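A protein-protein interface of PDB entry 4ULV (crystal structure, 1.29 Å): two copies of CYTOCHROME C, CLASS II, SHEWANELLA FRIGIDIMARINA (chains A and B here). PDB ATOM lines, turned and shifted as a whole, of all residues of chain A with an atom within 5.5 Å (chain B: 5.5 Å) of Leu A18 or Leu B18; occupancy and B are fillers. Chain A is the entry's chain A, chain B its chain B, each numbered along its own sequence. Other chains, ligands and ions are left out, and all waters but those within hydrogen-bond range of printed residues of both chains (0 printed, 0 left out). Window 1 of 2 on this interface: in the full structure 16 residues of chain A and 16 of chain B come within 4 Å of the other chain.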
ATOM      1  N   TYR A  11      -5.373 -15.696  19.826  1.00  0.00           N
ATOM      2  CA  TYR A  11      -3.947 -15.337  19.875  1.00  0.00           C
ATOM      3  C   TYR A  11      -3.090 -16.531  19.402  1.00  0.00           C
ATOM      4  O   TYR A  11      -2.218 -16.364  18.497  1.00  0.00           O
ATOM      5  CB  TYR A  11      -3.616 -14.915  21.282  1.00  0.00           C
ATOM      6  CG  TYR A  11      -2.191 -14.431  21.510  1.00  0.00           C
ATOM      7  CD1 TYR A  11      -1.852 -13.107  21.317  1.00  0.00           C
ATOM      8  CD2 TYR A  11      -1.206 -15.311  21.935  1.00  0.00           C
ATOM      9  CE1 TYR A  11      -0.566 -12.660  21.559  1.00  0.00           C
ATOM     10  CE2 TYR A  11       0.092 -14.884  22.135  1.00  0.00           C
ATOM     11  CZ  TYR A  11       0.398 -13.553  21.937  1.00  0.00           C
ATOM     12  OH  TYR A  11       1.668 -13.027  22.140  1.00  0.00           O
ATOM     13  N   GLN A  13      -3.930 -19.257  17.713  1.00  0.00           N
ATOM     14  CA  GLN A  13      -4.262 -19.564  16.299  1.00  0.00           C
ATOM     15  C   GLN A  13      -3.624 -18.598  15.275  1.00  0.00           C
ATOM     16  O   GLN A  13      -3.070 -19.004  14.247  1.00  0.00           O
ATOM     17  CB  GLN A  13      -5.770 -19.634  16.063  1.00  0.00           C
ATOM     18  CG  GLN A  13      -6.422 -20.787  16.817  1.00  0.00           C
ATOM     19  CD  GLN A  13      -7.945 -20.778  16.711  1.00  0.00           C
ATOM     20  OE1 GLN A  13      -8.558 -19.727  16.476  1.00  0.00           O
ATOM     21  NE2 GLN A  13      -8.544 -21.952  16.916  1.00  0.00           N
ATOM     22  N   ALA A  14      -3.644 -17.311  15.620  1.00  0.00           N
ATOM     23  CA  ALA A  14      -3.053 -16.275  14.777  1.00  0.00           C
ATOM     24  C   ALA A  14      -1.538 -16.550  14.630  1.00  0.00           C
ATOM     25  O   ALA A  14      -1.017 -16.511  13.527  1.00  0.00           O
ATOM     26  CB  ALA A  14      -3.240 -14.894  15.363  1.00  0.00           C
ATOM     27  N   ALA A  15      -0.927 -16.898  15.758  1.00  0.00           N
ATOM     28  CA  ALA A  15       0.544 -17.177  15.710  1.00  0.00           C
ATOM     29  C   ALA A  15       0.888 -18.389  14.866  1.00  0.00           C
ATOM     30  O   ALA A  15       1.793 -18.363  14.032  1.00  0.00           O
ATOM     31  CB  ALA A  15       1.050 -17.329  17.175  1.00  0.00           C
ATOM     32  N   PHE A  16       0.114 -19.448  15.075  1.00  0.00           N
ATOM     33  CA  PHE A  16       0.322 -20.653  14.265  1.00  0.00           C
ATOM     34  C   PHE A  16       0.102 -20.423  12.793  1.00  0.00           C
ATOM     35  O   PHE A  16       0.835 -20.972  11.955  1.00  0.00           O
ATOM     36  CB  PHE A  16      -0.501 -21.836  14.758  1.00  0.00           C
ATOM     37  CG  PHE A  16       0.008 -22.464  16.041  1.00  0.00           C
ATOM     38  CD1 PHE A  16       1.289 -23.016  16.135  1.00  0.00           C
ATOM     39  CD2 PHE A  16      -0.836 -22.557  17.126  1.00  0.00           C
ATOM     40  CE1 PHE A  16       1.673 -23.615  17.321  1.00  0.00           C
ATOM     41  CE2 PHE A  16      -0.464 -23.135  18.281  1.00  0.00           C
ATOM     42  CZ  PHE A  16       0.810 -23.638  18.399  1.00  0.00           C
ATOM     43  N   GLY A  17      -0.886 -19.619  12.430  1.00  0.00           N
ATOM     44  CA  GLY A  17      -1.031 -19.306  11.053  1.00  0.00           C
ATOM     45  C   GLY A  17       0.170 -18.635  10.418  1.00  0.00           C
ATOM     46  O   GLY A  17       0.526 -18.858   9.272  1.00  0.00           O
ATOM     47  N   LEU A  18       0.696 -17.688  11.165  1.00  0.00           N
ATOM     48  CA  LEU A  18       1.912 -16.971  10.700  1.00  0.00           C
ATOM     49  C   LEU A  18       3.136 -17.921  10.580  1.00  0.00           C
ATOM     50  O   LEU A  18       3.887 -17.820   9.605  1.00  0.00           O
ATOM     51  CB  LEU A  18       2.229 -15.776  11.546  1.00  0.00           C
ATOM     52  CG  LEU A  18       1.169 -14.678  11.606  1.00  0.00           C
ATOM     53  CD1 LEU A  18       1.683 -13.685  12.621  1.00  0.00           C
ATOM     54  CD2 LEU A  18       0.923 -14.040  10.286  1.00  0.00           C
ATOM     55  N   ILE A  19       3.222 -18.798  11.552  1.00  0.00           N
ATOM     56  CA  ILE A  19       4.307 -19.822  11.515  1.00  0.00           C
ATOM     57  C   ILE A  19       4.127 -20.628  10.237  1.00  0.00           C
ATOM     58  O   ILE A  19       5.105 -20.893   9.479  1.00  0.00           O
ATOM     59  CB  ILE A  19       4.254 -20.702  12.746  1.00  0.00           C
ATOM     60  CG1 ILE A  19       4.712 -19.933  13.969  1.00  0.00           C
ATOM     61  CG2 ILE A  19       5.041 -21.994  12.576  1.00  0.00           C
ATOM     62  CD1 ILE A  19       4.427 -20.616  15.270  1.00  0.00           C
ATOM     63  N   ALA A  20       2.889 -21.086   9.991  1.00  0.00           N
ATOM     64  CA  ALA A  20       2.612 -21.997   8.826  1.00  0.00           C
ATOM     65  C   ALA A  20       2.928 -21.287   7.513  1.00  0.00           C
ATOM     66  O   ALA A  20       3.480 -21.873   6.575  1.00  0.00           O
ATOM     67  CB  ALA A  20       1.202 -22.500   8.827  1.00  0.00           C
ATOM     68  N   TYR A  21       2.600 -20.013   7.401  1.00  0.00           N
ATOM     69  CA  TYR A  21       2.875 -19.292   6.168  1.00  0.00           C
ATOM     70  C   TYR A  21       4.389 -19.235   5.884  1.00  0.00           C
ATOM     71  O   TYR A  21       4.814 -19.471   4.767  1.00  0.00           O
ATOM     72  CB  TYR A  21       2.301 -17.860   6.215  1.00  0.00           C
ATOM     73  CG  TYR A  21       2.638 -17.007   5.034  1.00  0.00           C
ATOM     74  CD1 TYR A  21       1.882 -17.053   3.867  1.00  0.00           C
ATOM     75  CD2 TYR A  21       3.802 -16.208   5.044  1.00  0.00           C
ATOM     76  CE1 TYR A  21       2.204 -16.281   2.762  1.00  0.00           C
ATOM     77  CE2 TYR A  21       4.145 -15.434   3.933  1.00  0.00           C
ATOM     78  CZ  TYR A  21       3.362 -15.504   2.787  1.00  0.00           C
ATOM     79  OH  TYR A  21       3.651 -14.766   1.692  1.00  0.00           O
ATOM     80  N   ASN A  22       5.151 -18.932   6.910  1.00  0.00           N
ATOM     81  CA  ASN A  22       6.578 -18.806   6.723  1.00  0.00           C
ATOM     82  C   ASN A  22       7.262 -20.151   6.524  1.00  0.00           C
ATOM     83  O   ASN A  22       8.063 -20.285   5.604  1.00  0.00           O
ATOM     84  CB  ASN A  22       7.170 -18.012   7.922  1.00  0.00           C
ATOM     85  CG  ASN A  22       6.952 -16.517   7.790  1.00  0.00           C
ATOM     86  OD1 ASN A  22       7.691 -15.861   7.082  1.00  0.00           O
ATOM     87  ND2 ASN A  22       5.869 -16.017   8.378  1.00  0.00           N
ATOM     88  N   PHE A  23       6.871 -21.111   7.346  1.00  0.00           N
ATOM     89  CA  PHE A  23       7.441 -22.450   7.219  1.00  0.00           C
ATOM     90  C   PHE A  23       7.067 -23.074   5.876  1.00  0.00           C
ATOM     91  O   PHE A  23       7.867 -23.807   5.247  1.00  0.00           O
ATOM     92  CB  PHE A  23       6.936 -23.313   8.368  1.00  0.00           C
ATOM     93  CG  PHE A  23       7.671 -24.635   8.522  1.00  0.00           C
ATOM     94  CD1 PHE A  23       8.959 -24.649   8.969  1.00  0.00           C
ATOM     95  CD2 PHE A  23       7.042 -25.826   8.312  1.00  0.00           C
ATOM     96  CE1 PHE A  23       9.674 -25.815   9.120  1.00  0.00           C
ATOM     97  CE2 PHE A  23       7.718 -27.003   8.465  1.00  0.00           C
ATOM     98  CZ  PHE A  23       9.048 -27.001   8.899  1.00  0.00           C
ATOM     99  N   LEU A  51       8.539 -16.453  15.986  1.00  0.00           N
ATOM    100  CA  LEU A  51       7.113 -16.806  16.112  1.00  0.00           C
ATOM    101  C   LEU A  51       6.870 -17.985  16.993  1.00  0.00           C
ATOM    102  O   LEU A  51       5.855 -18.132  17.656  1.00  0.00           O
ATOM    103  CB  LEU A  51       6.438 -16.996  14.762  1.00  0.00           C
ATOM    104  CG  LEU A  51       6.209 -15.750  13.895  1.00  0.00           C
ATOM    105  CD1 LEU A  51       6.006 -16.108  12.416  1.00  0.00           C
ATOM    106  CD2 LEU A  51       5.045 -14.858  14.409  1.00  0.00           C
ATOM    107  N   ILE A  54       5.758 -17.445  20.492  1.00  0.00           N
ATOM    108  CA  ILE A  54       4.473 -16.663  20.693  1.00  0.00           C
ATOM    109  C   ILE A  54       3.265 -17.505  21.178  1.00  0.00           C
ATOM    110  O   ILE A  54       2.621 -17.126  22.140  1.00  0.00           O
ATOM    111  CB  ILE A  54       4.140 -15.881  19.448  1.00  0.00           C
ATOM    112  CG1 ILE A  54       5.215 -14.878  19.053  1.00  0.00           C
ATOM    113  CG2 ILE A  54       2.774 -15.127  19.578  1.00  0.00           C
ATOM    114  CD1 ILE A  54       5.576 -13.894  20.042  1.00  0.00           C
ATOM    115  N   TYR B  11      -3.441 -12.569   7.129  1.00  0.00           N
ATOM    116  CA  TYR B  11      -2.029 -12.559   7.519  1.00  0.00           C
ATOM    117  C   TYR B  11      -1.661 -11.232   8.225  1.00  0.00           C
ATOM    118  O   TYR B  11      -1.131 -11.230   9.317  1.00  0.00           O
ATOM    119  CB  TYR B  11      -1.176 -12.762   6.272  1.00  0.00           C
ATOM    120  CG  TYR B  11       0.287 -12.896   6.532  1.00  0.00           C
ATOM    121  CD1 TYR B  11       0.808 -14.125   6.922  1.00  0.00           C
ATOM    122  CD2 TYR B  11       1.167 -11.840   6.342  1.00  0.00           C
ATOM    123  CE1 TYR B  11       2.168 -14.296   7.130  1.00  0.00           C
ATOM    124  CE2 TYR B  11       2.565 -12.019   6.487  1.00  0.00           C
ATOM    125  CZ  TYR B  11       3.063 -13.260   6.926  1.00  0.00           C
ATOM    126  OH  TYR B  11       4.448 -13.478   7.139  1.00  0.00           O
ATOM    127  N   GLN B  13      -3.640  -8.853   9.385  1.00  0.00           N
ATOM    128  CA  GLN B  13      -4.472  -8.672  10.616  1.00  0.00           C
ATOM    129  C   GLN B  13      -3.969  -9.485  11.791  1.00  0.00           C
ATOM    130  O   GLN B  13      -3.892  -8.989  12.917  1.00  0.00           O
ATOM    131  CB  GLN B  13      -5.961  -8.988  10.342  1.00  0.00           C
ATOM    132  CG  GLN B  13      -6.659  -7.928   9.491  1.00  0.00           C
ATOM    133  CD  GLN B  13      -8.094  -8.219   9.159  1.00  0.00           C
ATOM    134  OE1 GLN B  13      -8.470  -9.396   9.178  1.00  0.00           O
ATOM    135  NE2 GLN B  13      -8.802  -7.216   8.643  1.00  0.00           N
ATOM    136  N   ALA B  14      -3.612 -10.752  11.517  1.00  0.00           N
ATOM    137  CA  ALA B  14      -3.161 -11.610  12.564  1.00  0.00           C
ATOM    138  C   ALA B  14      -1.889 -11.022  13.207  1.00  0.00           C
ATOM    139  O   ALA B  14      -1.716 -10.971  14.448  1.00  0.00           O
ATOM    140  CB  ALA B  14      -2.812 -12.968  12.008  1.00  0.00           C
ATOM    141  N   ALA B  15      -0.934 -10.596  12.354  1.00  0.00           N
ATOM    142  CA  ALA B  15       0.348 -10.026  12.844  1.00  0.00           C
ATOM    143  C   ALA B  15       0.094  -8.783  13.670  1.00  0.00           C
ATOM    144  O   ALA B  15       0.667  -8.600  14.731  1.00  0.00           O
ATOM    145  CB  ALA B  15       1.215  -9.705  11.663  1.00  0.00           C
ATOM    146  N   PHE B  16      -0.784  -7.877  13.188  1.00  0.00           N
ATOM    147  CA  PHE B  16      -1.017  -6.652  13.984  1.00  0.00           C
ATOM    148  C   PHE B  16      -1.732  -6.979  15.275  1.00  0.00           C
ATOM    149  O   PHE B  16      -1.485  -6.309  16.270  1.00  0.00           O
ATOM    150  CB  PHE B  16      -1.803  -5.663  13.139  1.00  0.00           C
ATOM    151  CG  PHE B  16      -0.972  -4.863  12.207  1.00  0.00           C
ATOM    152  CD1 PHE B  16       0.118  -4.089  12.692  1.00  0.00           C
ATOM    153  CD2 PHE B  16      -1.261  -4.824  10.865  1.00  0.00           C
ATOM    154  CE1 PHE B  16       0.881  -3.339  11.856  1.00  0.00           C
ATOM    155  CE2 PHE B  16      -0.489  -4.078  10.019  1.00  0.00           C
ATOM    156  CZ  PHE B  16       0.569  -3.316  10.522  1.00  0.00           C
ATOM    157  N   GLY B  17      -2.635  -7.974  15.298  1.00  0.00           N
ATOM    158  CA  GLY B  17      -3.192  -8.319  16.598  1.00  0.00           C
ATOM    159  C   GLY B  17      -2.183  -8.793  17.613  1.00  0.00           C
ATOM    160  O   GLY B  17      -2.212  -8.475  18.792  1.00  0.00           O
ATOM    161  N   LEU B  18      -1.243  -9.594  17.123  1.00  0.00           N
ATOM    162  CA  LEU B  18      -0.148 -10.037  17.978  1.00  0.00           C
ATOM    163  C   LEU B  18       0.734  -8.862  18.452  1.00  0.00           C
ATOM    164  O   LEU B  18       1.146  -8.797  19.632  1.00  0.00           O
ATOM    165  CB  LEU B  18       0.679 -11.133  17.278  1.00  0.00           C
ATOM    166  CG  LEU B  18      -0.036 -12.424  16.914  1.00  0.00           C
ATOM    167  CD1 LEU B  18       0.959 -13.318  16.191  1.00  0.00           C
ATOM    168  CD2 LEU B  18      -0.639 -13.136  18.087  1.00  0.00           C
ATOM    169  N   ILE B  19       1.007  -7.975  17.502  1.00  0.00           N
ATOM    170  CA  ILE B  19       1.800  -6.758  17.847  1.00  0.00           C
ATOM    171  C   ILE B  19       1.095  -5.967  18.949  1.00  0.00           C
ATOM    172  O   ILE B  19       1.720  -5.574  19.926  1.00  0.00           O
ATOM    173  CB  ILE B  19       2.007  -5.915  16.615  1.00  0.00           C
ATOM    174  CG1 ILE B  19       3.005  -6.556  15.690  1.00  0.00           C
ATOM    175  CG2 ILE B  19       2.437  -4.472  16.934  1.00  0.00           C
ATOM    176  CD1 ILE B  19       3.046  -5.943  14.332  1.00  0.00           C
ATOM    177  N   ALA B  20      -0.224  -5.785  18.806  1.00  0.00           N
ATOM    178  CA  ALA B  20      -0.989  -4.940  19.756  1.00  0.00           C
ATOM    179  C   ALA B  20      -0.994  -5.561  21.138  1.00  0.00           C
ATOM    180  O   ALA B  20      -0.878  -4.876  22.162  1.00  0.00           O
ATOM    181  CB  ALA B  20      -2.382  -4.712  19.229  1.00  0.00           C
ATOM    182  N   TYR B  21      -1.115  -6.881  21.199  1.00  0.00           N
ATOM    183  CA  TYR B  21      -1.168  -7.541  22.489  1.00  0.00           C
ATOM    184  C   TYR B  21       0.163  -7.360  23.244  1.00  0.00           C
ATOM    185  O   TYR B  21       0.213  -7.008  24.442  1.00  0.00           O
ATOM    186  CB  TYR B  21      -1.470  -9.028  22.320  1.00  0.00           C
ATOM    187  CG  TYR B  21      -1.448  -9.830  23.591  1.00  0.00           C
ATOM    188  CD1 TYR B  21      -2.574  -9.970  24.366  1.00  0.00           C
ATOM    189  CD2 TYR B  21      -0.275 -10.486  24.026  1.00  0.00           C
ATOM    190  CE1 TYR B  21      -2.585 -10.700  25.513  1.00  0.00           C
ATOM    191  CE2 TYR B  21      -0.269 -11.184  25.185  1.00  0.00           C
ATOM    192  CZ  TYR B  21      -1.434 -11.322  25.934  1.00  0.00           C
ATOM    193  OH  TYR B  21      -1.471 -12.025  27.104  1.00  0.00           O
ATOM    194  N   ASN B  22       1.276  -7.592  22.545  1.00  0.00           N
ATOM    195  CA  ASN B  22       2.579  -7.478  23.134  1.00  0.00           C
ATOM    196  C   ASN B  22       2.926  -6.008  23.430  1.00  0.00           C
ATOM    197  O   ASN B  22       3.496  -5.688  24.504  1.00  0.00           O
ATOM    198  CB  ASN B  22       3.632  -8.161  22.245  1.00  0.00           C
ATOM    199  CG  ASN B  22       3.568  -9.662  22.377  1.00  0.00           C
ATOM    200  OD1 ASN B  22       4.131 -10.230  23.324  1.00  0.00           O
ATOM    201  ND2 ASN B  22       2.747 -10.316  21.500  1.00  0.00           N
ATOM    202  N   PHE B  23       2.627  -5.135  22.497  1.00  0.00           N
ATOM    203  CA  PHE B  23       2.884  -3.695  22.705  1.00  0.00           C
ATOM    204  C   PHE B  23       2.046  -3.165  23.874  1.00  0.00           C
ATOM    205  O   PHE B  23       2.560  -2.347  24.673  1.00  0.00           O
ATOM    206  CB  PHE B  23       2.598  -2.915  21.420  1.00  0.00           C
ATOM    207  CG  PHE B  23       3.120  -1.499  21.429  1.00  0.00           C
ATOM    208  CD1 PHE B  23       4.458  -1.258  21.309  1.00  0.00           C
ATOM    209  CD2 PHE B  23       2.242  -0.453  21.476  1.00  0.00           C
ATOM    210  CE1 PHE B  23       4.912   0.012  21.282  1.00  0.00           C
ATOM    211  CE2 PHE B  23       2.714   0.835  21.515  1.00  0.00           C
ATOM    212  CZ  PHE B  23       4.037   1.065  21.411  1.00  0.00           C
ATOM    213  N   LEU B  51       7.813  -9.264  15.349  1.00  0.00           N
ATOM    214  CA  LEU B  51       6.554  -9.227  14.684  1.00  0.00           C
ATOM    215  C   LEU B  51       6.419  -8.090  13.694  1.00  0.00           C
ATOM    216  O   LEU B  51       5.691  -8.145  12.695  1.00  0.00           O
ATOM    217  CB  LEU B  51       5.421  -9.197  15.700  1.00  0.00           C
ATOM    218  CG  LEU B  51       5.168 -10.411  16.568  1.00  0.00           C
ATOM    219  CD1 LEU B  51       4.319 -10.022  17.769  1.00  0.00           C
ATOM    220  CD2 LEU B  51       4.461 -11.472  15.726  1.00  0.00           C
ATOM    221  N   ILE B  54       6.727  -8.670   9.990  1.00  0.00           N
ATOM    222  CA  ILE B  54       5.728  -9.578   9.357  1.00  0.00           C
ATOM    223  C   ILE B  54       4.683  -8.873   8.458  1.00  0.00           C
ATOM    224  O   ILE B  54       4.474  -9.275   7.337  1.00  0.00           O
ATOM    225  CB  ILE B  54       5.058 -10.463  10.412  1.00  0.00           C
ATOM    226  CG1 ILE B  54       6.047 -11.309  11.247  1.00  0.00           C
ATOM    227  CG2 ILE B  54       4.048 -11.411   9.810  1.00  0.00           C
ATOM    228  CD1 ILE B  54       6.954 -12.171  10.486  1.00  0.00           C
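O of Leu A18 sits at hydrogen-bond distance from ND2 of Asn A22.
O of Leu B18 is in hydrogen-bond range of ND2 of Asn B22 (2.9 Å).
Of the 14 printed residues of chain B, 7 touch a printed residue of chain A.
Hydrophobic or aromatic side chains of chain B within 4 Å of the printed part of chain A: Tyr B11, Ala B14, Leu B18, Tyr B21 and Leu B51.
Hydrophobic or aromatic side chains of chain A within 4 Å of the printed part of chain B: Tyr A11, Ala A14, Leu A18, Tyr A21 and Leu A51.
Among the printed residues, 11 pairs touch across the chains.
OH of Tyr A11 sits at hydrogen-bond distance from ND2 of Asn B22, at 3.0 Å.
The side-chain amide nitrogen of Asn A22 is in hydrogen-bond range of the side-chain hydroxyl of Tyr B11 (3.2 Å).
Of chain B, only Tyr B11 (3.4 Å), Ala B15 (3.9 Å) and Leu B18 (3.7 Å) come within 4 Å of Leu A18.
Of chain A, only Tyr A11 (3.5 Å), Ala A15 (3.9 Å) and Leu A18 (3.7 Å) come within 4 Å of Leu B18.
Printed residues of chain B within 4 Å of Ala A14: Ala B14.
Of the printed residues of chain B, Ala A15 touches Leu B18 (3.9 Å).
Of the printed residues of chain A, Tyr B21 touches Tyr A11.
Of the printed residues of chain A, Ala B14 touches Ala A14 (3.9 Å).
Tyr A11 touches Leu B18.
Tyr B21 touches Tyr A11.
Ala B14 touches Ala A14.
CA of Ala A15 touches CD1 of Leu B18 (3.9 Å).
CD1 of Tyr B11 touches CD2 of Leu A18, 3.4 Å away.
Leu A18 touches Ala B15 (CD1 to CA, 3.9 Å).
Leu A18 touches Leu B18.
Tyr A21 touches Tyr B11.
CD2 of Leu A51 touches CD2 of Leu B51, at 3.7 Å.
Tyr A11 touches Leu B18, and with the chains exchanged Leu A18 touches Tyr B11.
Tyr A11 touches Tyr B21, and with the chains exchanged Tyr A21 touches Tyr B11.
Ala A15 touches Leu B18, and with the chains exchanged Leu A18 touches Ala B15.
Leu B51 touches its own counterpart, Leu A51.
14 positions are printed for both chains.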
